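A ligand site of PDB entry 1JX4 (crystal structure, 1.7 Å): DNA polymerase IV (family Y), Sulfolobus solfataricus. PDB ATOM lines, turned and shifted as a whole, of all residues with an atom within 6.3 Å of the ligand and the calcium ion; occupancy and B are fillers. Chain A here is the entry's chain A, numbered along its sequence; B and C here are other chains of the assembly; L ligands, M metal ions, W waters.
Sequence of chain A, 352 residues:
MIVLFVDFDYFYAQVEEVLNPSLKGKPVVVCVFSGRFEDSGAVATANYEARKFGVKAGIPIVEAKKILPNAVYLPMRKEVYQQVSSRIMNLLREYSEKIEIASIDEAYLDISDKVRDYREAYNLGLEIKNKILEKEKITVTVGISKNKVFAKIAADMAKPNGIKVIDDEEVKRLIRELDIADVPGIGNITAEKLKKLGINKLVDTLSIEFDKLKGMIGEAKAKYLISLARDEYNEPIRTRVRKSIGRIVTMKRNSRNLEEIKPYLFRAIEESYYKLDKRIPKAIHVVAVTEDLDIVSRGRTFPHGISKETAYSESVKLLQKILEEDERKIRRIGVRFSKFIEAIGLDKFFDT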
ATOM      1  N   ASP A   7      -8.225 -12.008 -11.937  1.00  0.00           N
ATOM      2  CA  ASP A   7      -8.627 -10.806 -11.198  1.00  0.00           C
ATOM      3  C   ASP A   7      -9.727 -11.283 -10.234  1.00  0.00           C
ATOM      4  O   ASP A   7     -10.799 -11.701 -10.666  1.00  0.00           O
ATOM      5  CB  ASP A   7      -9.166  -9.828 -12.241  1.00  0.00           C
ATOM      6  CG  ASP A   7      -9.672  -8.523 -11.627  1.00  0.00           C
ATOM      7  OD1 ASP A   7     -10.206  -8.489 -10.479  1.00  0.00           O
ATOM      8  OD2 ASP A   7      -9.525  -7.526 -12.357  1.00  0.00           O
ATOM      9  N   PHE A   8      -9.436 -11.282  -8.936  1.00  0.00           N
ATOM     10  CA  PHE A   8     -10.428 -11.787  -7.980  1.00  0.00           C
ATOM     11  C   PHE A   8     -11.657 -10.872  -7.945  1.00  0.00           C
ATOM     12  O   PHE A   8     -11.545  -9.641  -7.987  1.00  0.00           O
ATOM     13  CB  PHE A   8      -9.839 -11.918  -6.536  1.00  0.00           C
ATOM     14  CG  PHE A   8      -8.487 -12.604  -6.426  1.00  0.00           C
ATOM     15  CD1 PHE A   8      -7.990 -13.397  -7.460  1.00  0.00           C
ATOM     16  CD2 PHE A   8      -7.679 -12.426  -5.267  1.00  0.00           C
ATOM     17  CE1 PHE A   8      -6.723 -13.997  -7.377  1.00  0.00           C
ATOM     18  CE2 PHE A   8      -6.406 -13.033  -5.175  1.00  0.00           C
ATOM     19  CZ  PHE A   8      -5.937 -13.811  -6.248  1.00  0.00           C
ATOM     20  N   ASP A   9     -12.846 -11.464  -7.830  1.00  0.00           N
ATOM     21  CA  ASP A   9     -14.044 -10.618  -7.861  1.00  0.00           C
ATOM     22  C   ASP A   9     -14.327  -9.860  -6.559  1.00  0.00           C
ATOM     23  O   ASP A   9     -14.277 -10.441  -5.468  1.00  0.00           O
ATOM     24  CB  ASP A   9     -15.268 -11.462  -8.264  1.00  0.00           C
ATOM     25  CG  ASP A   9     -15.088 -12.190  -9.631  1.00  0.00           C
ATOM     26  OD1 ASP A   9     -14.527 -11.564 -10.561  1.00  0.00           O
ATOM     27  OD2 ASP A   9     -15.536 -13.346  -9.779  1.00  0.00           O
ATOM     28  N   TYR A  10     -14.661  -8.576  -6.687  1.00  0.00           N
ATOM     29  CA  TYR A  10     -14.967  -7.693  -5.563  1.00  0.00           C
ATOM     30  C   TYR A  10     -14.284  -8.209  -4.311  1.00  0.00           C
ATOM     31  O   TYR A  10     -14.866  -8.330  -3.213  1.00  0.00           O
ATOM     32  CB  TYR A  10     -16.521  -7.593  -5.350  1.00  0.00           C
ATOM     33  CG  TYR A  10     -17.278  -8.882  -5.159  1.00  0.00           C
ATOM     34  CD1 TYR A  10     -17.777  -9.254  -3.880  1.00  0.00           C
ATOM     35  CD2 TYR A  10     -17.535  -9.743  -6.245  1.00  0.00           C
ATOM     36  CE1 TYR A  10     -18.522 -10.479  -3.690  1.00  0.00           C
ATOM     37  CE2 TYR A  10     -18.259 -10.975  -6.056  1.00  0.00           C
ATOM     38  CZ  TYR A  10     -18.739 -11.319  -4.770  1.00  0.00           C
ATOM     39  OH  TYR A  10     -19.329 -12.573  -4.572  1.00  0.00           O
ATOM     40  N   PHE A  11     -12.977  -8.402  -4.454  1.00  0.00           N
ATOM     41  CA  PHE A  11     -12.258  -9.125  -3.434  1.00  0.00           C
ATOM     42  C   PHE A  11     -12.504  -8.965  -1.952  1.00  0.00           C
ATOM     43  O   PHE A  11     -12.840  -9.960  -1.317  1.00  0.00           O
ATOM     44  CB  PHE A  11     -10.733  -9.067  -3.743  1.00  0.00           C
ATOM     45  CG  PHE A  11      -9.903 -10.056  -2.929  1.00  0.00           C
ATOM     46  CD1 PHE A  11     -10.209 -11.427  -2.942  1.00  0.00           C
ATOM     47  CD2 PHE A  11      -8.835  -9.637  -2.147  1.00  0.00           C
ATOM     48  CE1 PHE A  11      -9.469 -12.372  -2.174  1.00  0.00           C
ATOM     49  CE2 PHE A  11      -8.076 -10.568  -1.371  1.00  0.00           C
ATOM     50  CZ  PHE A  11      -8.409 -11.946  -1.401  1.00  0.00           C
ATOM     51  N   TYR A  12     -12.348  -7.768  -1.357  1.00  0.00           N
ATOM     52  CA  TYR A  12     -12.484  -7.671   0.079  1.00  0.00           C
ATOM     53  C   TYR A  12     -13.913  -8.036   0.528  1.00  0.00           C
ATOM     54  O   TYR A  12     -14.123  -8.701   1.572  1.00  0.00           O
ATOM     55  CB  TYR A  12     -12.175  -6.282   0.573  1.00  0.00           C
ATOM     56  CG  TYR A  12     -10.799  -5.756   0.251  1.00  0.00           C
ATOM     57  CD1 TYR A  12      -9.756  -6.607  -0.160  1.00  0.00           C
ATOM     58  CD2 TYR A  12     -10.513  -4.424   0.414  1.00  0.00           C
ATOM     59  CE1 TYR A  12      -8.469  -6.097  -0.378  1.00  0.00           C
ATOM     60  CE2 TYR A  12      -9.217  -3.929   0.229  1.00  0.00           C
ATOM     61  CZ  TYR A  12      -8.232  -4.772  -0.165  1.00  0.00           C
ATOM     62  OH  TYR A  12      -6.978  -4.249  -0.349  1.00  0.00           O
ATOM     63  N   ALA A  13     -14.884  -7.592  -0.263  1.00  0.00           N
ATOM     64  CA  ALA A  13     -16.261  -7.900   0.100  1.00  0.00           C
ATOM     65  C   ALA A  13     -16.500  -9.373  -0.080  1.00  0.00           C
ATOM     66  O   ALA A  13     -17.222  -9.954   0.736  1.00  0.00           O
ATOM     67  CB  ALA A  13     -17.242  -7.080  -0.740  1.00  0.00           C
ATOM     68  N   VAL A  32     -13.191   2.191   4.775  1.00  0.00           N
ATOM     69  CA  VAL A  32     -11.973   2.655   5.430  1.00  0.00           C
ATOM     70  C   VAL A  32     -12.462   3.834   6.265  1.00  0.00           C
ATOM     71  O   VAL A  32     -12.681   4.928   5.740  1.00  0.00           O
ATOM     72  CB  VAL A  32     -10.930   3.091   4.356  1.00  0.00           C
ATOM     73  CG1 VAL A  32      -9.624   3.398   5.024  1.00  0.00           C
ATOM     74  CG2 VAL A  32     -10.745   1.988   3.298  1.00  0.00           C
ATOM     75  N   VAL A  43     -15.313   4.289   0.879  1.00  0.00           N
ATOM     76  CA  VAL A  43     -15.563   2.889   0.548  1.00  0.00           C
ATOM     77  C   VAL A  43     -14.348   2.249  -0.167  1.00  0.00           C
ATOM     78  O   VAL A  43     -13.799   2.827  -1.155  1.00  0.00           O
ATOM     79  CB  VAL A  43     -16.809   2.786  -0.409  1.00  0.00           C
ATOM     80  CG1 VAL A  43     -16.977   1.311  -0.916  1.00  0.00           C
ATOM     81  CG2 VAL A  43     -18.011   3.303   0.390  1.00  0.00           C
ATOM     82  N   ALA A  44     -13.877   1.106   0.333  1.00  0.00           N
ATOM     83  CA  ALA A  44     -12.741   0.430  -0.343  1.00  0.00           C
ATOM     84  C   ALA A  44     -13.239  -0.386  -1.467  1.00  0.00           C
ATOM     85  O   ALA A  44     -12.588  -0.472  -2.523  1.00  0.00           O
ATOM     86  CB  ALA A  44     -11.987  -0.469   0.604  1.00  0.00           C
ATOM     87  N   THR A  45     -14.356  -1.081  -1.224  1.00  0.00           N
ATOM     88  CA  THR A  45     -14.976  -1.856  -2.269  1.00  0.00           C
ATOM     89  C   THR A  45     -16.356  -2.300  -1.813  1.00  0.00           C
ATOM     90  O   THR A  45     -16.668  -2.381  -0.605  1.00  0.00           O
ATOM     91  CB  THR A  45     -14.158  -3.081  -2.684  1.00  0.00           C
ATOM     92  OG1 THR A  45     -14.759  -3.684  -3.840  1.00  0.00           O
ATOM     93  CG2 THR A  45     -14.156  -4.087  -1.588  1.00  0.00           C
ATOM     94  N   ALA A  46     -17.205  -2.610  -2.764  1.00  0.00           N
ATOM     95  CA  ALA A  46     -18.531  -3.073  -2.401  1.00  0.00           C
ATOM     96  C   ALA A  46     -18.797  -4.262  -3.318  1.00  0.00           C
ATOM     97  O   ALA A  46     -18.176  -4.362  -4.384  1.00  0.00           O
ATOM     98  CB  ALA A  46     -19.535  -1.982  -2.645  1.00  0.00           C
ATOM     99  N   TYR A  48     -21.278  -6.719  -5.857  1.00  0.00           N
ATOM    100  CA  TYR A  48     -22.069  -6.234  -6.952  1.00  0.00           C
ATOM    101  C   TYR A  48     -23.491  -5.819  -6.590  1.00  0.00           C
ATOM    102  O   TYR A  48     -24.033  -4.976  -7.262  1.00  0.00           O
ATOM    103  CB  TYR A  48     -22.026  -7.221  -8.116  1.00  0.00           C
ATOM    104  CG  TYR A  48     -20.675  -7.131  -8.867  1.00  0.00           C
ATOM    105  CD1 TYR A  48     -19.509  -7.656  -8.309  1.00  0.00           C
ATOM    106  CD2 TYR A  48     -20.583  -6.497 -10.125  1.00  0.00           C
ATOM    107  CE1 TYR A  48     -18.299  -7.554  -8.958  1.00  0.00           C
ATOM    108  CE2 TYR A  48     -19.352  -6.402 -10.804  1.00  0.00           C
ATOM    109  CZ  TYR A  48     -18.218  -6.941 -10.213  1.00  0.00           C
ATOM    110  OH  TYR A  48     -16.994  -6.853 -10.903  1.00  0.00           O
ATOM    111  N   ARG A  51     -22.931  -2.209  -5.838  1.00  0.00           N
ATOM    112  CA  ARG A  51     -22.559  -1.421  -7.011  1.00  0.00           C
ATOM    113  C   ARG A  51     -23.698  -1.136  -7.961  1.00  0.00           C
ATOM    114  O   ARG A  51     -23.716  -0.055  -8.581  1.00  0.00           O
ATOM    115  CB  ARG A  51     -21.482  -2.100  -7.849  1.00  0.00           C
ATOM    116  CG  ARG A  51     -20.265  -2.452  -7.098  1.00  0.00           C
ATOM    117  CD  ARG A  51     -19.193  -3.001  -8.070  1.00  0.00           C
ATOM    118  NE  ARG A  51     -18.143  -3.560  -7.239  1.00  0.00           N
ATOM    119  CZ  ARG A  51     -16.973  -4.007  -7.666  1.00  0.00           C
ATOM    120  NH1 ARG A  51     -16.647  -3.967  -8.974  1.00  0.00           N
ATOM    121  NH2 ARG A  51     -16.146  -4.517  -6.769  1.00  0.00           N
ATOM    122  N   ALA A  57     -16.164   1.661  -4.878  1.00  0.00           N
ATOM    123  CA  ALA A  57     -14.888   2.105  -4.331  1.00  0.00           C
ATOM    124  C   ALA A  57     -14.678   3.594  -4.528  1.00  0.00           C
ATOM    125  O   ALA A  57     -14.900   4.127  -5.642  1.00  0.00           O
ATOM    126  CB  ALA A  57     -13.724   1.330  -4.998  1.00  0.00           C
ATOM    127  N   GLY A  58     -14.287   4.277  -3.466  1.00  0.00           N
ATOM    128  CA  GLY A  58     -13.927   5.672  -3.605  1.00  0.00           C
ATOM    129  C   GLY A  58     -14.868   6.739  -3.057  1.00  0.00           C
ATOM    130  O   GLY A  58     -14.443   7.806  -2.724  1.00  0.00           O
ATOM    131  N   MET A  76     -12.552  -2.401   6.829  1.00  0.00           N
ATOM    132  CA  MET A  76     -11.547  -3.137   6.009  1.00  0.00           C
ATOM    133  C   MET A  76     -10.637  -3.953   6.997  1.00  0.00           C
ATOM    134  O   MET A  76     -10.188  -3.388   7.979  1.00  0.00           O
ATOM    135  CB  MET A  76     -10.700  -2.106   5.275  1.00  0.00           C
ATOM    136  CG  MET A  76     -10.381  -2.358   3.764  1.00  0.00           C
ATOM    137  SD  MET A  76      -8.715  -1.482   3.198  1.00  0.00           S
ATOM    138  CE  MET A  76      -9.144  -1.165   1.327  1.00  0.00           C
ATOM    139  N   SER A 103      -1.004  -7.020  -7.729  1.00  0.00           N
ATOM    140  CA  SER A 103      -1.579  -6.364  -6.568  1.00  0.00           C
ATOM    141  C   SER A 103      -2.168  -7.449  -5.663  1.00  0.00           C
ATOM    142  O   SER A 103      -2.011  -8.639  -5.939  1.00  0.00           O
ATOM    143  CB  SER A 103      -2.687  -5.418  -7.007  1.00  0.00           C
ATOM    144  OG  SER A 103      -3.791  -6.167  -7.509  1.00  0.00           O
ATOM    145  N   ILE A 104      -2.890  -7.044  -4.633  1.00  0.00           N
ATOM    146  CA  ILE A 104      -3.465  -8.030  -3.736  1.00  0.00           C
ATOM    147  C   ILE A 104      -4.472  -8.931  -4.462  1.00  0.00           C
ATOM    148  O   ILE A 104      -4.759 -10.029  -3.970  1.00  0.00           O
ATOM    149  CB  ILE A 104      -4.117  -7.339  -2.504  1.00  0.00           C
ATOM    150  CG1 ILE A 104      -4.372  -8.366  -1.400  1.00  0.00           C
ATOM    151  CG2 ILE A 104      -5.305  -6.506  -2.958  1.00  0.00           C
ATOM    152  CD1 ILE A 104      -4.733  -7.728  -0.061  1.00  0.00           C
ATOM    153  N   ASP A 105      -5.016  -8.523  -5.630  1.00  0.00           N
ATOM    154  CA  ASP A 105      -5.961  -9.455  -6.230  1.00  0.00           C
ATOM    155  C   ASP A 105      -5.833  -9.643  -7.739  1.00  0.00           C
ATOM    156  O   ASP A 105      -6.784 -10.014  -8.427  1.00  0.00           O
ATOM    157  CB  ASP A 105      -7.388  -9.112  -5.827  1.00  0.00           C
ATOM    158  CG  ASP A 105      -8.006  -7.996  -6.699  1.00  0.00           C
ATOM    159  OD1 ASP A 105      -7.244  -7.106  -7.099  1.00  0.00           O
ATOM    160  OD2 ASP A 105      -9.245  -8.050  -6.942  1.00  0.00           O
ATOM    161  N   GLU A 106      -4.640  -9.389  -8.241  1.00  0.00           N
ATOM    162  CA  GLU A 106      -4.431  -9.578  -9.677  1.00  0.00           C
ATOM    163  C   GLU A 106      -3.108 -10.249  -9.943  1.00  0.00           C
ATOM    164  O   GLU A 106      -2.094  -9.898  -9.316  1.00  0.00           O
ATOM    165  CB  GLU A 106      -4.352  -8.235 -10.356  1.00  0.00           C
ATOM    166  CG  GLU A 106      -5.488  -7.315 -10.193  1.00  0.00           C
ATOM    167  CD  GLU A 106      -5.059  -5.989 -10.781  1.00  0.00           C
ATOM    168  OE1 GLU A 106      -4.120  -5.409 -10.235  1.00  0.00           O
ATOM    169  OE2 GLU A 106      -5.576  -5.535 -11.782  1.00  0.00           O
ATOM    170  N   LYS A 159     -15.805  -9.585 -16.076  1.00  0.00           N
ATOM    171  CA  LYS A 159     -16.085  -9.678 -14.626  1.00  0.00           C
ATOM    172  C   LYS A 159     -17.534  -9.298 -14.311  1.00  0.00           C
ATOM    173  O   LYS A 159     -18.142  -8.495 -15.037  1.00  0.00           O
ATOM    174  CB  LYS A 159     -15.111  -8.807 -13.807  1.00  0.00           C
ATOM    175  CG  LYS A 159     -15.219  -7.308 -14.092  1.00  0.00           C
ATOM    176  CD  LYS A 159     -14.267  -6.482 -13.177  1.00  0.00           C
ATOM    177  CE  LYS A 159     -12.829  -6.988 -13.191  1.00  0.00           C
ATOM    178  NZ  LYS A 159     -11.820  -6.050 -12.561  1.00  0.00           N
ATOM    179  P    DT B   5      -9.739  10.860   2.340  1.00  0.00           P
ATOM    180  OP1  DT B   5      -9.830  11.662   3.575  1.00  0.00           O
ATOM    181  OP2  DT B   5      -8.682  11.196   1.313  1.00  0.00           O
ATOM    182  O5'  DT B   5      -9.623   9.350   2.815  1.00  0.00           O
ATOM    183  C5'  DT B   5     -10.438   8.864   3.870  1.00  0.00           C
ATOM    184  C4'  DT B   5      -9.937   7.503   4.278  1.00  0.00           C
ATOM    185  O4'  DT B   5     -10.237   6.571   3.220  1.00  0.00           O
ATOM    186  C3'  DT B   5      -8.427   7.480   4.441  1.00  0.00           C
ATOM    187  O3'  DT B   5      -8.133   6.573   5.490  1.00  0.00           O
ATOM    188  C2'  DT B   5      -7.922   6.977   3.087  1.00  0.00           C
ATOM    189  C1'  DT B   5      -9.064   6.071   2.599  1.00  0.00           C
ATOM    190  N1   DT B   5      -9.352   6.075   1.137  1.00  0.00           N
ATOM    191  C2   DT B   5      -9.217   4.879   0.434  1.00  0.00           C
ATOM    192  O2   DT B   5      -8.846   3.857   0.924  1.00  0.00           O
ATOM    193  N3   DT B   5      -9.576   4.958  -0.879  1.00  0.00           N
ATOM    194  C4   DT B   5     -10.051   6.041  -1.553  1.00  0.00           C
ATOM    195  O4   DT B   5     -10.394   5.940  -2.736  1.00  0.00           O
ATOM    196  C5   DT B   5     -10.132   7.256  -0.793  1.00  0.00           C
ATOM    197  C7   DT B   5     -10.614   8.475  -1.505  1.00  0.00           C
ATOM    198  C6   DT B   5      -9.779   7.214   0.510  1.00  0.00           C
ATOM    199  P    DT B   6      -6.633   6.521   6.076  1.00  0.00           P
ATOM    200  OP1  DT B   6      -6.772   5.914   7.408  1.00  0.00           O
ATOM    201  OP2  DT B   6      -6.062   7.860   5.904  1.00  0.00           O
ATOM    202  O5'  DT B   6      -5.876   5.513   5.113  1.00  0.00           O
ATOM    203  C5'  DT B   6      -6.184   4.162   5.197  1.00  0.00           C
ATOM    204  C4'  DT B   6      -5.527   3.412   4.070  1.00  0.00           C
ATOM    205  O4'  DT B   6      -6.085   3.879   2.823  1.00  0.00           O
ATOM    206  C3'  DT B   6      -3.995   3.566   3.929  1.00  0.00           C
ATOM    207  O3'  DT B   6      -3.417   2.312   4.269  1.00  0.00           O
ATOM    208  C2'  DT B   6      -3.785   3.900   2.444  1.00  0.00           C
ATOM    209  C1'  DT B   6      -5.148   3.508   1.815  1.00  0.00           C
ATOM    210  N1   DT B   6      -5.526   4.228   0.576  1.00  0.00           N
ATOM    211  C2   DT B   6      -5.746   3.453  -0.556  1.00  0.00           C
ATOM    212  O2   DT B   6      -5.599   2.251  -0.559  1.00  0.00           O
ATOM    213  N3   DT B   6      -6.176   4.157  -1.649  1.00  0.00           N
ATOM    214  C4   DT B   6      -6.396   5.510  -1.735  1.00  0.00           C
ATOM    215  O4   DT B   6      -6.842   5.993  -2.756  1.00  0.00           O
ATOM    216  C5   DT B   6      -6.093   6.276  -0.538  1.00  0.00           C
ATOM    217  C7   DT B   6      -6.216   7.762  -0.566  1.00  0.00           C
ATOM    218  C6   DT B   6      -5.683   5.587   0.549  1.00  0.00           C
ATOM    219  P    DA C  13      -6.826  -1.174 -12.105  1.00  0.00           P
ATOM    220  OP1  DA C  13      -7.003  -2.306 -13.065  1.00  0.00           O
ATOM    221  OP2  DA C  13      -7.838  -0.075 -12.082  1.00  0.00           O
ATOM    222  O5'  DA C  13      -6.677  -1.813 -10.659  1.00  0.00           O
ATOM    223  C5'  DA C  13      -5.482  -2.539 -10.312  1.00  0.00           C
ATOM    224  C4'  DA C  13      -5.487  -2.852  -8.839  1.00  0.00           C
ATOM    225  O4'  DA C  13      -5.303  -1.624  -8.077  1.00  0.00           O
ATOM    226  C3'  DA C  13      -6.817  -3.445  -8.375  1.00  0.00           C
ATOM    227  C2'  DA C  13      -7.550  -2.238  -7.812  1.00  0.00           C
ATOM    228  C1'  DA C  13      -6.393  -1.448  -7.186  1.00  0.00           C
ATOM    229  N9   DA C  13      -6.659  -0.015  -7.017  1.00  0.00           N
ATOM    230  C8   DA C  13      -7.225   0.819  -7.923  1.00  0.00           C
ATOM    231  N7   DA C  13      -7.445   2.026  -7.466  1.00  0.00           N
ATOM    232  C5   DA C  13      -6.939   1.991  -6.177  1.00  0.00           C
ATOM    233  C6   DA C  13      -6.915   2.945  -5.147  1.00  0.00           C
ATOM    234  N6   DA C  13      -7.435   4.166  -5.257  1.00  0.00           N
ATOM    235  N1   DA C  13      -6.350   2.586  -3.978  1.00  0.00           N
ATOM    236  C2   DA C  13      -5.905   1.337  -3.833  1.00  0.00           C
ATOM    237  N3   DA C  13      -5.906   0.344  -4.714  1.00  0.00           N
ATOM    238  C4   DA C  13      -6.439   0.745  -5.886  1.00  0.00           C
HETATM  239  P1  LIG L   1     -12.743  -4.708  -9.269  1.00  0.00           P
HETATM  240  O1  LIG L   1     -11.953  -5.976  -9.635  1.00  0.00           O
HETATM  241  O2  LIG L   1     -12.613  -3.490 -10.068  1.00  0.00           O
HETATM  242  O3  LIG L   1     -14.158  -5.273  -9.112  1.00  0.00           O
HETATM  243  P2  LIG L   1     -12.118  -5.166  -6.442  1.00  0.00           P
HETATM  244  O4  LIG L   1     -11.885  -6.629  -6.855  1.00  0.00           O
HETATM  245  O5  LIG L   1     -13.256  -4.784  -5.586  1.00  0.00           O
HETATM  246  O6  LIG L   1     -12.064  -4.401  -7.860  1.00  0.00           O
HETATM  247  O7  LIG L   1     -10.787  -4.504  -5.834  1.00  0.00           O
HETATM  248  C1  LIG L   1      -9.594  -5.237  -5.480  1.00  0.00           C
HETATM  249  C2  LIG L   1      -9.053  -4.636  -4.181  1.00  0.00           C
HETATM  250  O8  LIG L   1      -8.628  -3.354  -4.697  1.00  0.00           O
HETATM  251  C3  LIG L   1     -10.243  -4.411  -3.242  1.00  0.00           C
HETATM  252  C4  LIG L   1      -9.795  -3.059  -2.723  1.00  0.00           C
HETATM  253  C5  LIG L   1      -8.904  -2.376  -3.718  1.00  0.00           C
HETATM  254  N1  LIG L   1      -9.431  -1.064  -4.144  1.00  0.00           N
HETATM  255  C6  LIG L   1     -10.034  -0.704  -5.356  1.00  0.00           C
HETATM  256  N2  LIG L   1     -10.316   0.564  -5.421  1.00  0.00           N
HETATM  257  C7  LIG L   1      -9.931   1.068  -4.192  1.00  0.00           C
HETATM  258  C8  LIG L   1      -9.999   2.371  -3.621  1.00  0.00           C
HETATM  259  N3  LIG L   1     -10.537   3.419  -4.235  1.00  0.00           N
HETATM  260  N4  LIG L   1      -9.485   2.513  -2.348  1.00  0.00           N
HETATM  261  C9  LIG L   1      -8.968   1.457  -1.673  1.00  0.00           C
HETATM  262  N5  LIG L   1      -8.883   0.199  -2.080  1.00  0.00           N
HETATM  263  C10 LIG L   1      -9.387   0.087  -3.380  1.00  0.00           C
HETATM  264 CA    CA M   1     -10.734  -7.574  -8.526  1.00  0.00          CA
HETATM  265  O   HOH W   1      -8.868  -5.877  -9.096  1.00  0.00           O
HETATM  266  O   HOH W   2     -13.450  -1.969  -5.583  1.00  0.00           O
HETATM  267  O   HOH W   3     -14.638  -2.776 -11.750  1.00  0.00           O
HETATM  268  O   HOH W   4      -7.026  -1.317  -0.517  1.00  0.00           O
HETATM  269  O   HOH W   5     -14.901  -7.563  -9.421  1.00  0.00           O
HETATM  270  O   HOH W   6     -11.169   0.726  -7.935  1.00  0.00           O
HETATM  271  O   HOH W   7     -12.885  -1.168  -8.417  1.00  0.00           O
HETATM  272  O   HOH W   8     -10.192  -3.563 -11.319  1.00  0.00           O
HETATM  273  O   HOH W   9     -11.359   3.228  -7.188  1.00  0.00           O
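The side-chain hydroxyl (OG1) of Thr 45 is in hydrogen-bond range of an oxygen (O5) of the ligand, 2.6 Å away. The guanidinium group (NH1) of Arg 51 is in salt-bridge range of an oxygen (O3) of the ligand (2.8 Å). O4 of DT 5 of chain B sits at hydrogen-bond distance from a nitrogen (N3) of the ligand, at 2.9 Å. O2 of the ligand lies within salt-bridge range of NZ of Lys 159 (3.7 Å). The backbone NH (N) of Phe 11 sits close to an oxygen (O4) of the ligand (3.2 Å). N6 of DA 13 of chain C is in hydrogen-bond range of a nitrogen (N3) of the ligand, at 3.4 Å. An oxygen (O4) of the ligand sits close to the backbone NH (N) of Tyr 10, at 3.4 Å.
OD2 of Asp 7 lies within salt-bridge range of NZ of Lys 159 (2.7 Å). The side-chain hydroxyl (OG) of Ser 103 lies close to the backbone NH (N) of Asp 105 (3.3 Å). The guanidinium group (NH2) of Arg 51 is in hydrogen-bond range of the side-chain hydroxyl (OG1) of Thr 45, 3.3 Å away. The guanidinium group of Arg 51 sits at hydrogen-bond distance from the side-chain hydroxyl of Tyr 48 (3.5 Å). O of Ala 46 is in hydrogen-bond range of NE of Arg 51, at 3.0 Å. The backbone NH (N) of Gly 58 is in hydrogen-bond range of the backbone carbonyl oxygen (O) of Val 43 (2.8 Å).
CE2 of Tyr 12 touches C4 of the ligand (3.1 Å). Ala 44 touches the ligand (O to C10, 3.4 Å). Tyr 48 touches the ligand (OH to O3, 3.7 Å). Ala 57 touches the ligand (CB to N2, 3.5 Å). N of Gly 58 touches N3 of the ligand, at 3.9 Å. Met 76 touches the ligand. DT 6 of chain B touches the ligand.
Along chain A the residues within 4 Å of the calcium ion span positions 7 to 105.
The calcium ion is bound by the side-chain carboxylate of Asp 7 (2.2 Å), the side-chain carboxylate of Asp 105 (2.2 Å), an oxygen (O4) of the ligand (2.2 Å), the backbone carbonyl oxygen of Phe 8 (2.3 Å), an oxygen (O1) of the ligand (2.3 Å) and water W1 (2.6 Å). The calcium ion has six donor atoms within binding distance.
Water W5 lies within hydrogen-bond range of O3 of the ligand, OH of Tyr 48 and N of Tyr 10. Water W8 lies within hydrogen-bond range of an oxygen (O2) of the ligand and the side-chain amino group of Lys 159. Water W2 lies within hydrogen-bond range of the side-chain hydroxyl of Thr 45 and an oxygen (O5) of the ligand. Water W4 lies within hydrogen-bond range of N5 of the ligand and OH of Tyr 12.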
